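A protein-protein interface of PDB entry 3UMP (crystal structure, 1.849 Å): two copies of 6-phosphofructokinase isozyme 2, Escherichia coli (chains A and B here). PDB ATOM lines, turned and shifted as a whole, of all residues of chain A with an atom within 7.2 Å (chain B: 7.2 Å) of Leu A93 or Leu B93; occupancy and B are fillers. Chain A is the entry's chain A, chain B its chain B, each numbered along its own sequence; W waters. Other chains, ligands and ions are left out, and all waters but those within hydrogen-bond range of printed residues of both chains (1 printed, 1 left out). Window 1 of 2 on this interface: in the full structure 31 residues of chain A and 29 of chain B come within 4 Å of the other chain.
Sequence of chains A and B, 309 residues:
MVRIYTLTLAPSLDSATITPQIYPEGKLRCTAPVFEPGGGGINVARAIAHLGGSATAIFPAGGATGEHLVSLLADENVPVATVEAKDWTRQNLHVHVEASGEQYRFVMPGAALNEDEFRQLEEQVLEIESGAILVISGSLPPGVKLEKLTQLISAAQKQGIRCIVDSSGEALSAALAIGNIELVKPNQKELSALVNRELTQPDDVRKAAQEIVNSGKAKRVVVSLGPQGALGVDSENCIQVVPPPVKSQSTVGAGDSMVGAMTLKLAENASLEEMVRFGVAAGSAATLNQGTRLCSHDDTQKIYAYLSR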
ATOM      1  N   LEU A  13     -11.075   2.588   7.568  1.00  0.00           N
ATOM      2  CA  LEU A  13     -10.716   3.843   6.942  1.00  0.00           C
ATOM      3  C   LEU A  13     -11.803   4.089   5.908  1.00  0.00           C
ATOM      4  O   LEU A  13     -11.822   3.446   4.859  1.00  0.00           O
ATOM      5  CB  LEU A  13      -9.351   3.743   6.257  1.00  0.00           C
ATOM      6  CG  LEU A  13      -8.856   5.034   5.596  1.00  0.00           C
ATOM      7  CD1 LEU A  13      -8.459   6.043   6.665  1.00  0.00           C
ATOM      8  CD2 LEU A  13      -7.685   4.748   4.661  1.00  0.00           C
ATOM      9  N   ASP A  14     -12.732   4.988   6.211  1.00  0.00           N
ATOM     10  CA  ASP A  14     -13.884   5.170   5.331  1.00  0.00           C
ATOM     11  C   ASP A  14     -13.607   6.164   4.205  1.00  0.00           C
ATOM     12  O   ASP A  14     -12.919   7.168   4.404  1.00  0.00           O
ATOM     13  CB  ASP A  14     -15.115   5.590   6.134  1.00  0.00           C
ATOM     14  CG  ASP A  14     -15.506   4.559   7.169  1.00  0.00           C
ATOM     15  OD1 ASP A  14     -15.092   3.387   7.022  1.00  0.00           O
ATOM     16  OD2 ASP A  14     -16.230   4.918   8.120  1.00  0.00           O
ATOM     17  N   SER A  15     -14.140   5.866   3.023  1.00  0.00           N
ATOM     18  CA  SER A  15     -14.057   6.781   1.890  1.00  0.00           C
ATOM     19  C   SER A  15     -15.379   7.508   1.741  1.00  0.00           C
ATOM     20  O   SER A  15     -16.428   6.885   1.742  1.00  0.00           O
ATOM     21  CB  SER A  15     -13.771   6.021   0.596  1.00  0.00           C
ATOM     22  OG  SER A  15     -12.421   5.611   0.515  1.00  0.00           O
ATOM     23  N   ALA A  16     -15.329   8.826   1.600  1.00  0.00           N
ATOM     24  CA  ALA A  16     -16.535   9.575   1.286  1.00  0.00           C
ATOM     25  C   ALA A  16     -16.381  10.185  -0.102  1.00  0.00           C
ATOM     26  O   ALA A  16     -15.443  10.953  -0.354  1.00  0.00           O
ATOM     27  CB  ALA A  16     -16.776  10.661   2.328  1.00  0.00           C
ATOM     28  N   THR A  17     -17.299   9.847  -1.003  1.00  0.00           N
ATOM     29  CA  THR A  17     -17.196  10.300  -2.388  1.00  0.00           C
ATOM     30  C   THR A  17     -18.515  10.917  -2.844  1.00  0.00           C
ATOM     31  O   THR A  17     -19.534  10.795  -2.158  1.00  0.00           O
ATOM     32  CB  THR A  17     -16.796   9.139  -3.332  1.00  0.00           C
ATOM     33  OG1 THR A  17     -16.620   9.641  -4.662  1.00  0.00           O
ATOM     34  CG2 THR A  17     -17.894   8.048  -3.351  1.00  0.00           C
ATOM     35  N   CYS A  30     -17.256   8.498  -9.505  1.00  0.00           N
ATOM     36  CA  CYS A  30     -17.216   9.055  -8.165  1.00  0.00           C
ATOM     37  C   CYS A  30     -15.979   9.932  -7.995  1.00  0.00           C
ATOM     38  O   CYS A  30     -14.935   9.646  -8.580  1.00  0.00           O
ATOM     39  CB  CYS A  30     -17.206   7.913  -7.159  1.00  0.00           C
ATOM     40  SG  CYS A  30     -18.779   7.008  -7.170  1.00  0.00           S
ATOM     41  N   PRO A  33     -11.939  10.168  -3.255  1.00  0.00           N
ATOM     42  CA  PRO A  33     -12.573  10.144  -1.933  1.00  0.00           C
ATOM     43  C   PRO A  33     -11.817  10.935  -0.868  1.00  0.00           C
ATOM     44  O   PRO A  33     -10.588  11.057  -0.918  1.00  0.00           O
ATOM     45  CB  PRO A  33     -12.583   8.657  -1.573  1.00  0.00           C
ATOM     46  CG  PRO A  33     -11.425   8.073  -2.356  1.00  0.00           C
ATOM     47  CD  PRO A  33     -11.378   8.860  -3.643  1.00  0.00           C
ATOM     48  N   GLU A  36     -11.868   9.220   6.108  1.00  0.00           N
ATOM     49  CA  GLU A  36     -12.250   9.541   7.470  1.00  0.00           C
ATOM     50  C   GLU A  36     -12.102   8.309   8.367  1.00  0.00           C
ATOM     51  O   GLU A  36     -12.307   7.173   7.918  1.00  0.00           O
ATOM     52  CB  GLU A  36     -13.697  10.042   7.502  1.00  0.00           C
ATOM     53  CG  GLU A  36     -14.461   9.758   6.207  1.00  0.00           C
ATOM     54  CD  GLU A  36     -15.826  10.433   6.148  1.00  0.00           C
ATOM     55  OE1 GLU A  36     -15.894  11.658   6.399  1.00  0.00           O
ATOM     56  OE2 GLU A  36     -16.822   9.732   5.843  1.00  0.00           O
ATOM     57  N   GLN A  91     -12.200  -0.766   4.420  1.00  0.00           N
ATOM     58  CA  GLN A  91     -12.788   0.525   4.055  1.00  0.00           C
ATOM     59  C   GLN A  91     -14.278   0.412   3.799  1.00  0.00           C
ATOM     60  O   GLN A  91     -14.714  -0.440   3.021  1.00  0.00           O
ATOM     61  CB  GLN A  91     -12.146   1.065   2.780  1.00  0.00           C
ATOM     62  CG  GLN A  91     -10.623   1.146   2.802  1.00  0.00           C
ATOM     63  CD  GLN A  91     -10.093   2.002   1.667  1.00  0.00           C
ATOM     64  OE1 GLN A  91     -10.241   3.225   1.681  1.00  0.00           O
ATOM     65  NE2 GLN A  91      -9.493   1.362   0.668  1.00  0.00           N
ATOM     66  N   ASN A  92     -15.056   1.273   4.446  1.00  0.00           N
ATOM     67  CA  ASN A  92     -16.465   1.414   4.105  1.00  0.00           C
ATOM     68  C   ASN A  92     -16.633   2.589   3.144  1.00  0.00           C
ATOM     69  O   ASN A  92     -15.711   3.391   2.981  1.00  0.00           O
ATOM     70  CB  ASN A  92     -17.324   1.608   5.356  1.00  0.00           C
ATOM     71  CG  ASN A  92     -17.358   0.362   6.232  1.00  0.00           C
ATOM     72  OD1 ASN A  92     -17.166  -0.746   5.741  1.00  0.00           O
ATOM     73  ND2 ASN A  92     -17.601   0.543   7.524  1.00  0.00           N
ATOM     74  N   LEU A  93     -17.798   2.680   2.509  1.00  0.00           N
ATOM     75  CA  LEU A  93     -17.992   3.696   1.482  1.00  0.00           C
ATOM     76  C   LEU A  93     -19.237   4.513   1.756  1.00  0.00           C
ATOM     77  O   LEU A  93     -20.332   3.957   1.931  1.00  0.00           O
ATOM     78  CB  LEU A  93     -18.092   3.066   0.089  1.00  0.00           C
ATOM     79  CG  LEU A  93     -18.256   4.056  -1.078  1.00  0.00           C
ATOM     80  CD1 LEU A  93     -17.085   5.018  -1.163  1.00  0.00           C
ATOM     81  CD2 LEU A  93     -18.447   3.344  -2.415  1.00  0.00           C
ATOM     82  N   HIS A  94     -19.062   5.835   1.764  1.00  0.00           N
ATOM     83  CA  HIS A  94     -20.154   6.774   1.918  1.00  0.00           C
ATOM     84  C   HIS A  94     -20.281   7.542   0.610  1.00  0.00           C
ATOM     85  O   HIS A  94     -19.329   8.203   0.181  1.00  0.00           O
ATOM     86  CB  HIS A  94     -19.827   7.735   3.068  1.00  0.00           C
ATOM     87  CG  HIS A  94     -20.860   8.795   3.285  1.00  0.00           C
ATOM     88  ND1 HIS A  94     -20.950   9.922   2.495  1.00  0.00           N
ATOM     89  CD2 HIS A  94     -21.841   8.907   4.213  1.00  0.00           C
ATOM     90  CE1 HIS A  94     -21.945  10.680   2.922  1.00  0.00           C
ATOM     91  NE2 HIS A  94     -22.502  10.084   3.963  1.00  0.00           N
ATOM     92  N   VAL A  95     -21.444   7.434  -0.030  1.00  0.00           N
ATOM     93  CA  VAL A  95     -21.672   8.091  -1.315  1.00  0.00           C
ATOM     94  C   VAL A  95     -22.750   9.164  -1.218  1.00  0.00           C
ATOM     95  O   VAL A  95     -23.902   8.865  -0.912  1.00  0.00           O
ATOM     96  CB  VAL A  95     -22.097   7.092  -2.400  1.00  0.00           C
ATOM     97  CG1 VAL A  95     -22.237   7.807  -3.749  1.00  0.00           C
ATOM     98  CG2 VAL A  95     -21.099   5.943  -2.499  1.00  0.00           C
ATOM     99  N   TYR A 104     -25.673   7.355   0.633  1.00  0.00           N
ATOM    100  CA  TYR A 104     -25.724   5.899   0.697  1.00  0.00           C
ATOM    101  C   TYR A 104     -24.509   5.396   1.445  1.00  0.00           C
ATOM    102  O   TYR A 104     -23.390   5.864   1.214  1.00  0.00           O
ATOM    103  CB  TYR A 104     -25.770   5.302  -0.709  1.00  0.00           C
ATOM    104  CG  TYR A 104     -27.074   5.599  -1.406  1.00  0.00           C
ATOM    105  CD1 TYR A 104     -28.106   4.669  -1.420  1.00  0.00           C
ATOM    106  CD2 TYR A 104     -27.289   6.826  -2.007  1.00  0.00           C
ATOM    107  CE1 TYR A 104     -29.303   4.949  -2.035  1.00  0.00           C
ATOM    108  CE2 TYR A 104     -28.485   7.114  -2.623  1.00  0.00           C
ATOM    109  CZ  TYR A 104     -29.488   6.171  -2.632  1.00  0.00           C
ATOM    110  OH  TYR A 104     -30.678   6.456  -3.249  1.00  0.00           O
ATOM    111  N   ARG A 105     -24.725   4.430   2.331  1.00  0.00           N
ATOM    112  CA  ARG A 105     -23.677   3.990   3.233  1.00  0.00           C
ATOM    113  C   ARG A 105     -23.503   2.483   3.110  1.00  0.00           C
ATOM    114  O   ARG A 105     -24.392   1.721   3.489  1.00  0.00           O
ATOM    115  CB  ARG A 105     -24.052   4.357   4.667  1.00  0.00           C
ATOM    116  CG  ARG A 105     -24.322   5.843   4.834  1.00  0.00           C
ATOM    117  CD  ARG A 105     -25.139   6.131   6.079  1.00  0.00           C
ATOM    118  NE  ARG A 105     -24.406   5.836   7.301  1.00  0.00           N
ATOM    119  CZ  ARG A 105     -24.966   5.749   8.507  1.00  0.00           C
ATOM    120  NH1 ARG A 105     -26.273   5.929   8.663  1.00  0.00           N
ATOM    121  NH2 ARG A 105     -24.215   5.476   9.558  1.00  0.00           N
ATOM    122  N   PHE A 106     -22.360   2.065   2.585  1.00  0.00           N
ATOM    123  CA  PHE A 106     -22.081   0.644   2.416  1.00  0.00           C
ATOM    124  C   PHE A 106     -21.107   0.216   3.498  1.00  0.00           C
ATOM    125  O   PHE A 106     -19.964   0.670   3.532  1.00  0.00           O
ATOM    126  CB  PHE A 106     -21.563   0.373   1.002  1.00  0.00           C
ATOM    127  CG  PHE A 106     -22.505   0.854  -0.066  1.00  0.00           C
ATOM    128  CD1 PHE A 106     -22.342   2.104  -0.644  1.00  0.00           C
ATOM    129  CD2 PHE A 106     -23.597   0.087  -0.435  1.00  0.00           C
ATOM    130  CE1 PHE A 106     -23.236   2.566  -1.605  1.00  0.00           C
ATOM    131  CE2 PHE A 106     -24.495   0.534  -1.386  1.00  0.00           C
ATOM    132  CZ  PHE A 106     -24.315   1.786  -1.975  1.00  0.00           C
ATOM    133  N   VAL A 107     -21.604  -0.627   4.402  1.00  0.00           N
ATOM    134  CA  VAL A 107     -20.873  -1.039   5.591  1.00  0.00           C
ATOM    135  C   VAL A 107     -20.466  -2.512   5.465  1.00  0.00           C
ATOM    136  O   VAL A 107     -21.322  -3.401   5.420  1.00  0.00           O
ATOM    137  CB  VAL A 107     -21.719  -0.836   6.876  1.00  0.00           C
ATOM    138  CG1 VAL A 107     -20.923  -1.260   8.117  1.00  0.00           C
ATOM    139  CG2 VAL A 107     -22.161   0.609   7.004  1.00  0.00           C
ATOM    140  N   MET A 108     -19.160  -2.743   5.389  1.00  0.00           N
ATOM    141  CA  MET A 108     -18.596  -4.070   5.188  1.00  0.00           C
ATOM    142  C   MET A 108     -17.858  -4.448   6.464  1.00  0.00           C
ATOM    143  O   MET A 108     -17.635  -3.583   7.314  1.00  0.00           O
ATOM    144  CB  MET A 108     -17.660  -4.052   3.981  1.00  0.00           C
ATOM    145  CG  MET A 108     -18.363  -4.399   2.683  1.00  0.00           C
ATOM    146  SD  MET A 108     -17.393  -3.889   1.265  1.00  0.00           S
ATOM    147  CE  MET A 108     -17.411  -2.102   1.546  1.00  0.00           C
ATOM    148  N   LEU B  13      -7.919  -2.729  -6.841  1.00  0.00           N
ATOM    149  CA  LEU B  13      -8.349  -3.959  -6.211  1.00  0.00           C
ATOM    150  C   LEU B  13      -9.817  -3.744  -5.928  1.00  0.00           C
ATOM    151  O   LEU B  13     -10.175  -3.022  -5.002  1.00  0.00           O
ATOM    152  CB  LEU B  13      -7.595  -4.214  -4.903  1.00  0.00           C
ATOM    153  CG  LEU B  13      -7.976  -5.558  -4.283  1.00  0.00           C
ATOM    154  CD1 LEU B  13      -7.483  -6.683  -5.198  1.00  0.00           C
ATOM    155  CD2 LEU B  13      -7.414  -5.695  -2.874  1.00  0.00           C
ATOM    156  N   ASP B  14     -10.671  -4.345  -6.746  1.00  0.00           N
ATOM    157  CA  ASP B  14     -12.104  -4.116  -6.631  1.00  0.00           C
ATOM    158  C   ASP B  14     -12.750  -5.027  -5.587  1.00  0.00           C
ATOM    159  O   ASP B  14     -12.353  -6.182  -5.423  1.00  0.00           O
ATOM    160  CB  ASP B  14     -12.774  -4.285  -7.991  1.00  0.00           C
ATOM    161  CG  ASP B  14     -12.335  -3.230  -8.987  1.00  0.00           C
ATOM    162  OD1 ASP B  14     -11.747  -2.213  -8.554  1.00  0.00           O
ATOM    163  OD2 ASP B  14     -12.583  -3.421 -10.197  1.00  0.00           O
ATOM    164  N   SER B  15     -13.729  -4.487  -4.866  1.00  0.00           N
ATOM    165  CA  SER B  15     -14.526  -5.271  -3.929  1.00  0.00           C
ATOM    166  C   SER B  15     -15.908  -5.562  -4.507  1.00  0.00           C
ATOM    167  O   SER B  15     -16.593  -4.659  -4.990  1.00  0.00           O
ATOM    168  CB  SER B  15     -14.695  -4.519  -2.615  1.00  0.00           C
ATOM    169  OG  SER B  15     -13.528  -4.610  -1.830  1.00  0.00           O
ATOM    170  N   ALA B  16     -16.316  -6.823  -4.456  1.00  0.00           N
ATOM    171  CA  ALA B  16     -17.666  -7.201  -4.863  1.00  0.00           C
ATOM    172  C   ALA B  16     -18.419  -7.673  -3.624  1.00  0.00           C
ATOM    173  O   ALA B  16     -17.991  -8.614  -2.938  1.00  0.00           O
ATOM    174  CB  ALA B  16     -17.619  -8.302  -5.908  1.00  0.00           C
ATOM    175  N   THR B  17     -19.523  -7.004  -3.320  1.00  0.00           N
ATOM    176  CA  THR B  17     -20.269  -7.312  -2.113  1.00  0.00           C
ATOM    177  C   THR B  17     -21.763  -7.459  -2.408  1.00  0.00           C
ATOM    178  O   THR B  17     -22.233  -7.113  -3.501  1.00  0.00           O
ATOM    179  CB  THR B  17     -20.013  -6.260  -1.005  1.00  0.00           C
ATOM    180  OG1 THR B  17     -20.660  -6.668   0.196  1.00  0.00           O
ATOM    181  CG2 THR B  17     -20.548  -4.873  -1.429  1.00  0.00           C
ATOM    182  N   CYS B  30     -23.281  -5.009   4.260  1.00  0.00           N
ATOM    183  CA  CYS B  30     -22.780  -5.703   3.082  1.00  0.00           C
ATOM    184  C   CYS B  30     -21.927  -6.907   3.481  1.00  0.00           C
ATOM    185  O   CYS B  30     -21.190  -6.860   4.471  1.00  0.00           O
ATOM    186  CB  CYS B  30     -21.956  -4.748   2.226  1.00  0.00           C
ATOM    187  SG  CYS B  30     -22.927  -3.382   1.525  1.00  0.00           S
ATOM    188  N   PRO B  33     -16.440  -8.788   1.294  1.00  0.00           N
ATOM    189  CA  PRO B  33     -16.253  -8.665  -0.156  1.00  0.00           C
ATOM    190  C   PRO B  33     -15.355  -9.741  -0.761  1.00  0.00           C
ATOM    191  O   PRO B  33     -14.464 -10.290  -0.090  1.00  0.00           O
ATOM    192  CB  PRO B  33     -15.593  -7.290  -0.313  1.00  0.00           C
ATOM    193  CG  PRO B  33     -14.911  -7.053   1.001  1.00  0.00           C
ATOM    194  CD  PRO B  33     -15.817  -7.678   2.035  1.00  0.00           C
ATOM    195  N   GLU B  36     -11.317  -8.676  -6.636  1.00  0.00           N
ATOM    196  CA  GLU B  36     -11.042  -9.035  -8.029  1.00  0.00           C
ATOM    197  C   GLU B  36     -10.142  -7.981  -8.670  1.00  0.00           C
ATOM    198  O   GLU B  36     -10.197  -6.807  -8.296  1.00  0.00           O
ATOM    199  CB  GLU B  36     -12.350  -9.179  -8.819  1.00  0.00           C
ATOM    200  CG  GLU B  36     -13.140  -7.881  -8.950  1.00  0.00           C
ATOM    201  CD  GLU B  36     -14.653  -8.090  -9.002  1.00  0.00           C
ATOM    202  OE1 GLU B  36     -15.100  -9.236  -9.227  1.00  0.00           O
ATOM    203  OE2 GLU B  36     -15.394  -7.095  -8.812  1.00  0.00           O
ATOM    204  N   GLN B  91      -9.409   1.075  -4.383  1.00  0.00           N
ATOM    205  CA  GLN B  91     -10.476   0.085  -4.470  1.00  0.00           C
ATOM    206  C   GLN B  91     -11.756   0.696  -5.016  1.00  0.00           C
ATOM    207  O   GLN B  91     -12.209   1.731  -4.518  1.00  0.00           O
ATOM    208  CB  GLN B  91     -10.783  -0.475  -3.085  1.00  0.00           C
ATOM    209  CG  GLN B  91      -9.601  -1.126  -2.394  1.00  0.00           C
ATOM    210  CD  GLN B  91     -10.027  -1.954  -1.196  1.00  0.00           C
ATOM    211  OE1 GLN B  91      -9.991  -1.487  -0.058  1.00  0.00           O
ATOM    212  NE2 GLN B  91     -10.438  -3.193  -1.452  1.00  0.00           N
ATOM    213  N   ASN B  92     -12.329   0.059  -6.034  1.00  0.00           N
ATOM    214  CA  ASN B  92     -13.685   0.366  -6.457  1.00  0.00           C
ATOM    215  C   ASN B  92     -14.649  -0.649  -5.841  1.00  0.00           C
ATOM    216  O   ASN B  92     -14.227  -1.708  -5.379  1.00  0.00           O
ATOM    217  CB  ASN B  92     -13.799   0.359  -7.990  1.00  0.00           C
ATOM    218  CG  ASN B  92     -13.023   1.508  -8.640  1.00  0.00           C
ATOM    219  OD1 ASN B  92     -12.877   2.575  -8.049  1.00  0.00           O
ATOM    220  ND2 ASN B  92     -12.511   1.280  -9.847  1.00  0.00           N
ATOM    221  N   LEU B  93     -15.938  -0.320  -5.847  1.00  0.00           N
ATOM    222  CA  LEU B  93     -16.942  -1.140  -5.180  1.00  0.00           C
ATOM    223  C   LEU B  93     -18.052  -1.571  -6.137  1.00  0.00           C
ATOM    224  O   LEU B  93     -18.648  -0.744  -6.828  1.00  0.00           O
ATOM    225  CB  LEU B  93     -17.540  -0.386  -3.987  1.00  0.00           C
ATOM    226  CG  LEU B  93     -18.567  -1.152  -3.137  1.00  0.00           C
ATOM    227  CD1 LEU B  93     -17.945  -2.374  -2.445  1.00  0.00           C
ATOM    228  CD2 LEU B  93     -19.262  -0.253  -2.105  1.00  0.00           C
ATOM    229  N   HIS B  94     -18.317  -2.875  -6.166  1.00  0.00           N
ATOM    230  CA  HIS B  94     -19.426  -3.445  -6.917  1.00  0.00           C
ATOM    231  C   HIS B  94     -20.426  -4.009  -5.902  1.00  0.00           C
ATOM    232  O   HIS B  94     -20.097  -4.899  -5.109  1.00  0.00           O
ATOM    233  CB  HIS B  94     -18.905  -4.537  -7.871  1.00  0.00           C
ATOM    234  CG  HIS B  94     -19.979  -5.265  -8.623  1.00  0.00           C
ATOM    235  ND1 HIS B  94     -20.764  -6.243  -8.044  1.00  0.00           N
ATOM    236  CD2 HIS B  94     -20.393  -5.175  -9.911  1.00  0.00           C
ATOM    237  CE1 HIS B  94     -21.618  -6.709  -8.934  1.00  0.00           C
ATOM    238  NE2 HIS B  94     -21.412  -6.079 -10.080  1.00  0.00           N
ATOM    239  N   VAL B  95     -21.639  -3.467  -5.904  1.00  0.00           N
ATOM    240  CA  VAL B  95     -22.661  -3.889  -4.942  1.00  0.00           C
ATOM    241  C   VAL B  95     -23.788  -4.603  -5.666  1.00  0.00           C
ATOM    242  O   VAL B  95     -24.410  -4.037  -6.559  1.00  0.00           O
ATOM    243  CB  VAL B  95     -23.267  -2.693  -4.185  1.00  0.00           C
ATOM    244  CG1 VAL B  95     -24.308  -3.176  -3.137  1.00  0.00           C
ATOM    245  CG2 VAL B  95     -22.177  -1.890  -3.513  1.00  0.00           C
ATOM    246  N   TYR B 104     -24.669  -2.154  -8.570  1.00  0.00           N
ATOM    247  CA  TYR B 104     -24.271  -0.753  -8.526  1.00  0.00           C
ATOM    248  C   TYR B 104     -22.757  -0.718  -8.494  1.00  0.00           C
ATOM    249  O   TYR B 104     -22.117  -1.475  -7.751  1.00  0.00           O
ATOM    250  CB  TYR B 104     -24.864  -0.053  -7.302  1.00  0.00           C
ATOM    251  CG  TYR B 104     -26.367   0.127  -7.390  1.00  0.00           C
ATOM    252  CD1 TYR B 104     -26.917   1.320  -7.853  1.00  0.00           C
ATOM    253  CD2 TYR B 104     -27.236  -0.899  -7.032  1.00  0.00           C
ATOM    254  CE1 TYR B 104     -28.291   1.488  -7.953  1.00  0.00           C
ATOM    255  CE2 TYR B 104     -28.614  -0.743  -7.136  1.00  0.00           C
ATOM    256  CZ  TYR B 104     -29.133   0.454  -7.597  1.00  0.00           C
ATOM    257  OH  TYR B 104     -30.500   0.626  -7.690  1.00  0.00           O
ATOM    258  N   ARG B 105     -22.182   0.157  -9.307  1.00  0.00           N
ATOM    259  CA  ARG B 105     -20.747   0.143  -9.528  1.00  0.00           C
ATOM    260  C   ARG B 105     -20.214   1.536  -9.269  1.00  0.00           C
ATOM    261  O   ARG B 105     -20.576   2.471  -9.974  1.00  0.00           O
ATOM    262  CB  ARG B 105     -20.447  -0.246 -10.979  1.00  0.00           C
ATOM    263  CG  ARG B 105     -21.092  -1.550 -11.401  1.00  0.00           C
ATOM    264  CD  ARG B 105     -21.213  -1.658 -12.911  1.00  0.00           C
ATOM    265  NE  ARG B 105     -19.923  -1.748 -13.585  1.00  0.00           N
ATOM    266  CZ  ARG B 105     -19.765  -1.617 -14.902  1.00  0.00           C
ATOM    267  NH1 ARG B 105     -20.808  -1.380 -15.681  1.00  0.00           N
ATOM    268  NH2 ARG B 105     -18.563  -1.727 -15.440  1.00  0.00           N
ATOM    269  N   PHE B 106     -19.370   1.666  -8.255  1.00  0.00           N
ATOM    270  CA  PHE B 106     -18.821   2.958  -7.862  1.00  0.00           C
ATOM    271  C   PHE B 106     -17.351   2.988  -8.247  1.00  0.00           C
ATOM    272  O   PHE B 106     -16.541   2.219  -7.722  1.00  0.00           O
ATOM    273  CB  PHE B 106     -19.033   3.176  -6.361  1.00  0.00           C
ATOM    274  CG  PHE B 106     -20.482   3.076  -5.949  1.00  0.00           C
ATOM    275  CD1 PHE B 106     -21.006   1.879  -5.483  1.00  0.00           C
ATOM    276  CD2 PHE B 106     -21.328   4.171  -6.070  1.00  0.00           C
ATOM    277  CE1 PHE B 106     -22.338   1.780  -5.137  1.00  0.00           C
ATOM    278  CE2 PHE B 106     -22.663   4.082  -5.721  1.00  0.00           C
ATOM    279  CZ  PHE B 106     -23.170   2.882  -5.253  1.00  0.00           C
ATOM    280  N   VAL B 107     -17.027   3.866  -9.192  1.00  0.00           N
ATOM    281  CA  VAL B 107     -15.694   3.918  -9.775  1.00  0.00           C
ATOM    282  C   VAL B 107     -14.987   5.201  -9.356  1.00  0.00           C
ATOM    283  O   VAL B 107     -15.409   6.300  -9.724  1.00  0.00           O
ATOM    284  CB  VAL B 107     -15.760   3.835 -11.310  1.00  0.00           C
ATOM    285  CG1 VAL B 107     -14.358   3.856 -11.895  1.00  0.00           C
ATOM    286  CG2 VAL B 107     -16.518   2.570 -11.742  1.00  0.00           C
ATOM    287  N   MET B 108     -13.922   5.048  -8.573  1.00  0.00           N
ATOM    288  CA  MET B 108     -13.135   6.179  -8.096  1.00  0.00           C
ATOM    289  C   MET B 108     -11.771   6.166  -8.788  1.00  0.00           C
ATOM    290  O   MET B 108     -11.413   5.162  -9.421  1.00  0.00           O
ATOM    291  CB  MET B 108     -12.996   6.094  -6.578  1.00  0.00           C
ATOM    292  CG  MET B 108     -14.251   6.522  -5.839  1.00  0.00           C
ATOM    293  SD  MET B 108     -14.271   5.946  -4.137  1.00  0.00           S
ATOM    294  CE  MET B 108     -14.596   4.191  -4.399  1.00  0.00           C
HETATM  295  O   HOH W   1      -9.531   2.850  -1.884  1.00  0.00           O
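The backbone carbonyl oxygen (O) of Val B107 lies within hydrogen-bond range of the backbone NH (N) of Cys A30 (2.9 Å).
The side-chain amide oxygen (OE1) of Gln B91 is in hydrogen-bond range of the side-chain amide nitrogen (NE2) of Gln A91 (3.0 Å).
N of Cys B30 lies within hydrogen-bond range of O of Val A107, 2.8 Å away.
The side-chain hydroxyl (OG) of Ser A15 is in hydrogen-bond range of the side-chain amide oxygen (OE1) of Gln A91, 3.4 Å away.
The side-chain amide oxygen (OD1) of Asn A92 is in hydrogen-bond range of the backbone NH (N) of Met A108 (2.8 Å).
The backbone NH (N) of Val A95 lies within hydrogen-bond range of the backbone carbonyl oxygen (O) of Tyr A104 (2.8 Å).
NE2 of Gln B91 is in hydrogen-bond range of OG of Ser B15 (3.4 Å).
The backbone carbonyl oxygen (O) of Leu B93 is in hydrogen-bond range of the backbone NH (N) of Phe B106, 2.9 Å away.
The backbone NH (N) of Val B95 lies within hydrogen-bond range of the backbone carbonyl oxygen (O) of Tyr B104.
Cys A30 touches Phe B106.
Met B108 touches Cys A30.
Pro A33 touches Met B108.
CD2 of Leu B93 touches CD2 of Leu A93, at 3.7 Å.
Phe B106 touches Leu A93 (CB to CD2, 3.99 Å).
Val A95 touches Phe B106 (CG2 to CD2, 3.99 Å).
Leu B93 touches Phe A106 (CD2 to CB, 3.9 Å).
CD2 of Phe A106 touches CG2 of Val B95, at 3.9 Å.
Phe A106 touches Phe B106.
CB of Cys B30 touches CG of Met A108 (3.6 Å).
Printed residues of chain B within 4 Å of Leu A93: Leu B93 and Phe B106.
Leu B93 touches just these residues of chain A: Leu A93 (3.7 Å) and Phe A106 (3.9 Å).
Of the printed residues of chain B, Met A108 touches Cys B30.
Of the printed residues of chain A, Met B108 touches Cys A30 and Pro A33.
Of the printed residues of chain B, Phe A106 touches Leu B93 (3.9 Å), Val B95 (3.9 Å) and Phe B106 (3.6 Å).
Of the printed residues of chain B, Cys A30 touches Phe B106 (3.9 Å), Val B107 (2.9 Å) and Met B108 (3.5 Å).
The nearest printed residue of chain B that does not touch Leu A93 is Met B108 (4.2 Å).
The nearest residue of chain A that does not touch Leu B93 is Met A108 (4.04 Å).
Of the 18 printed residues of chain A, 8 touch a printed residue of chain B.
Hydrophobic or aromatic side chains of chain A that line the printed part of chain B: Pro A33, Leu A93, Val A95, Phe A106 and Met A108.
Among the printed residues, 13 pairs touch across the chains.
Among the printed residues, no Asp or Glu carboxylate lies within 4 Å of a Lys or Arg side-chain nitrogen of the other chain.
Cys A30 touches Phe B106, but with the chains exchanged Phe A106 does not touch Cys B30 (4.03 Å).
Gln A91 touches its own counterpart, Gln B91.
Leu B93 touches its own counterpart, Leu A93.
Phe A106 touches its own counterpart, Phe B106.
Of the 13 pairs that touch across the chains among the printed residues, 11 have their exchanged pair printed and touching as well.
Water W1 bridges NE2 of Gln A91 (3.0 Å) and N of Gln B91 (3.1 Å).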
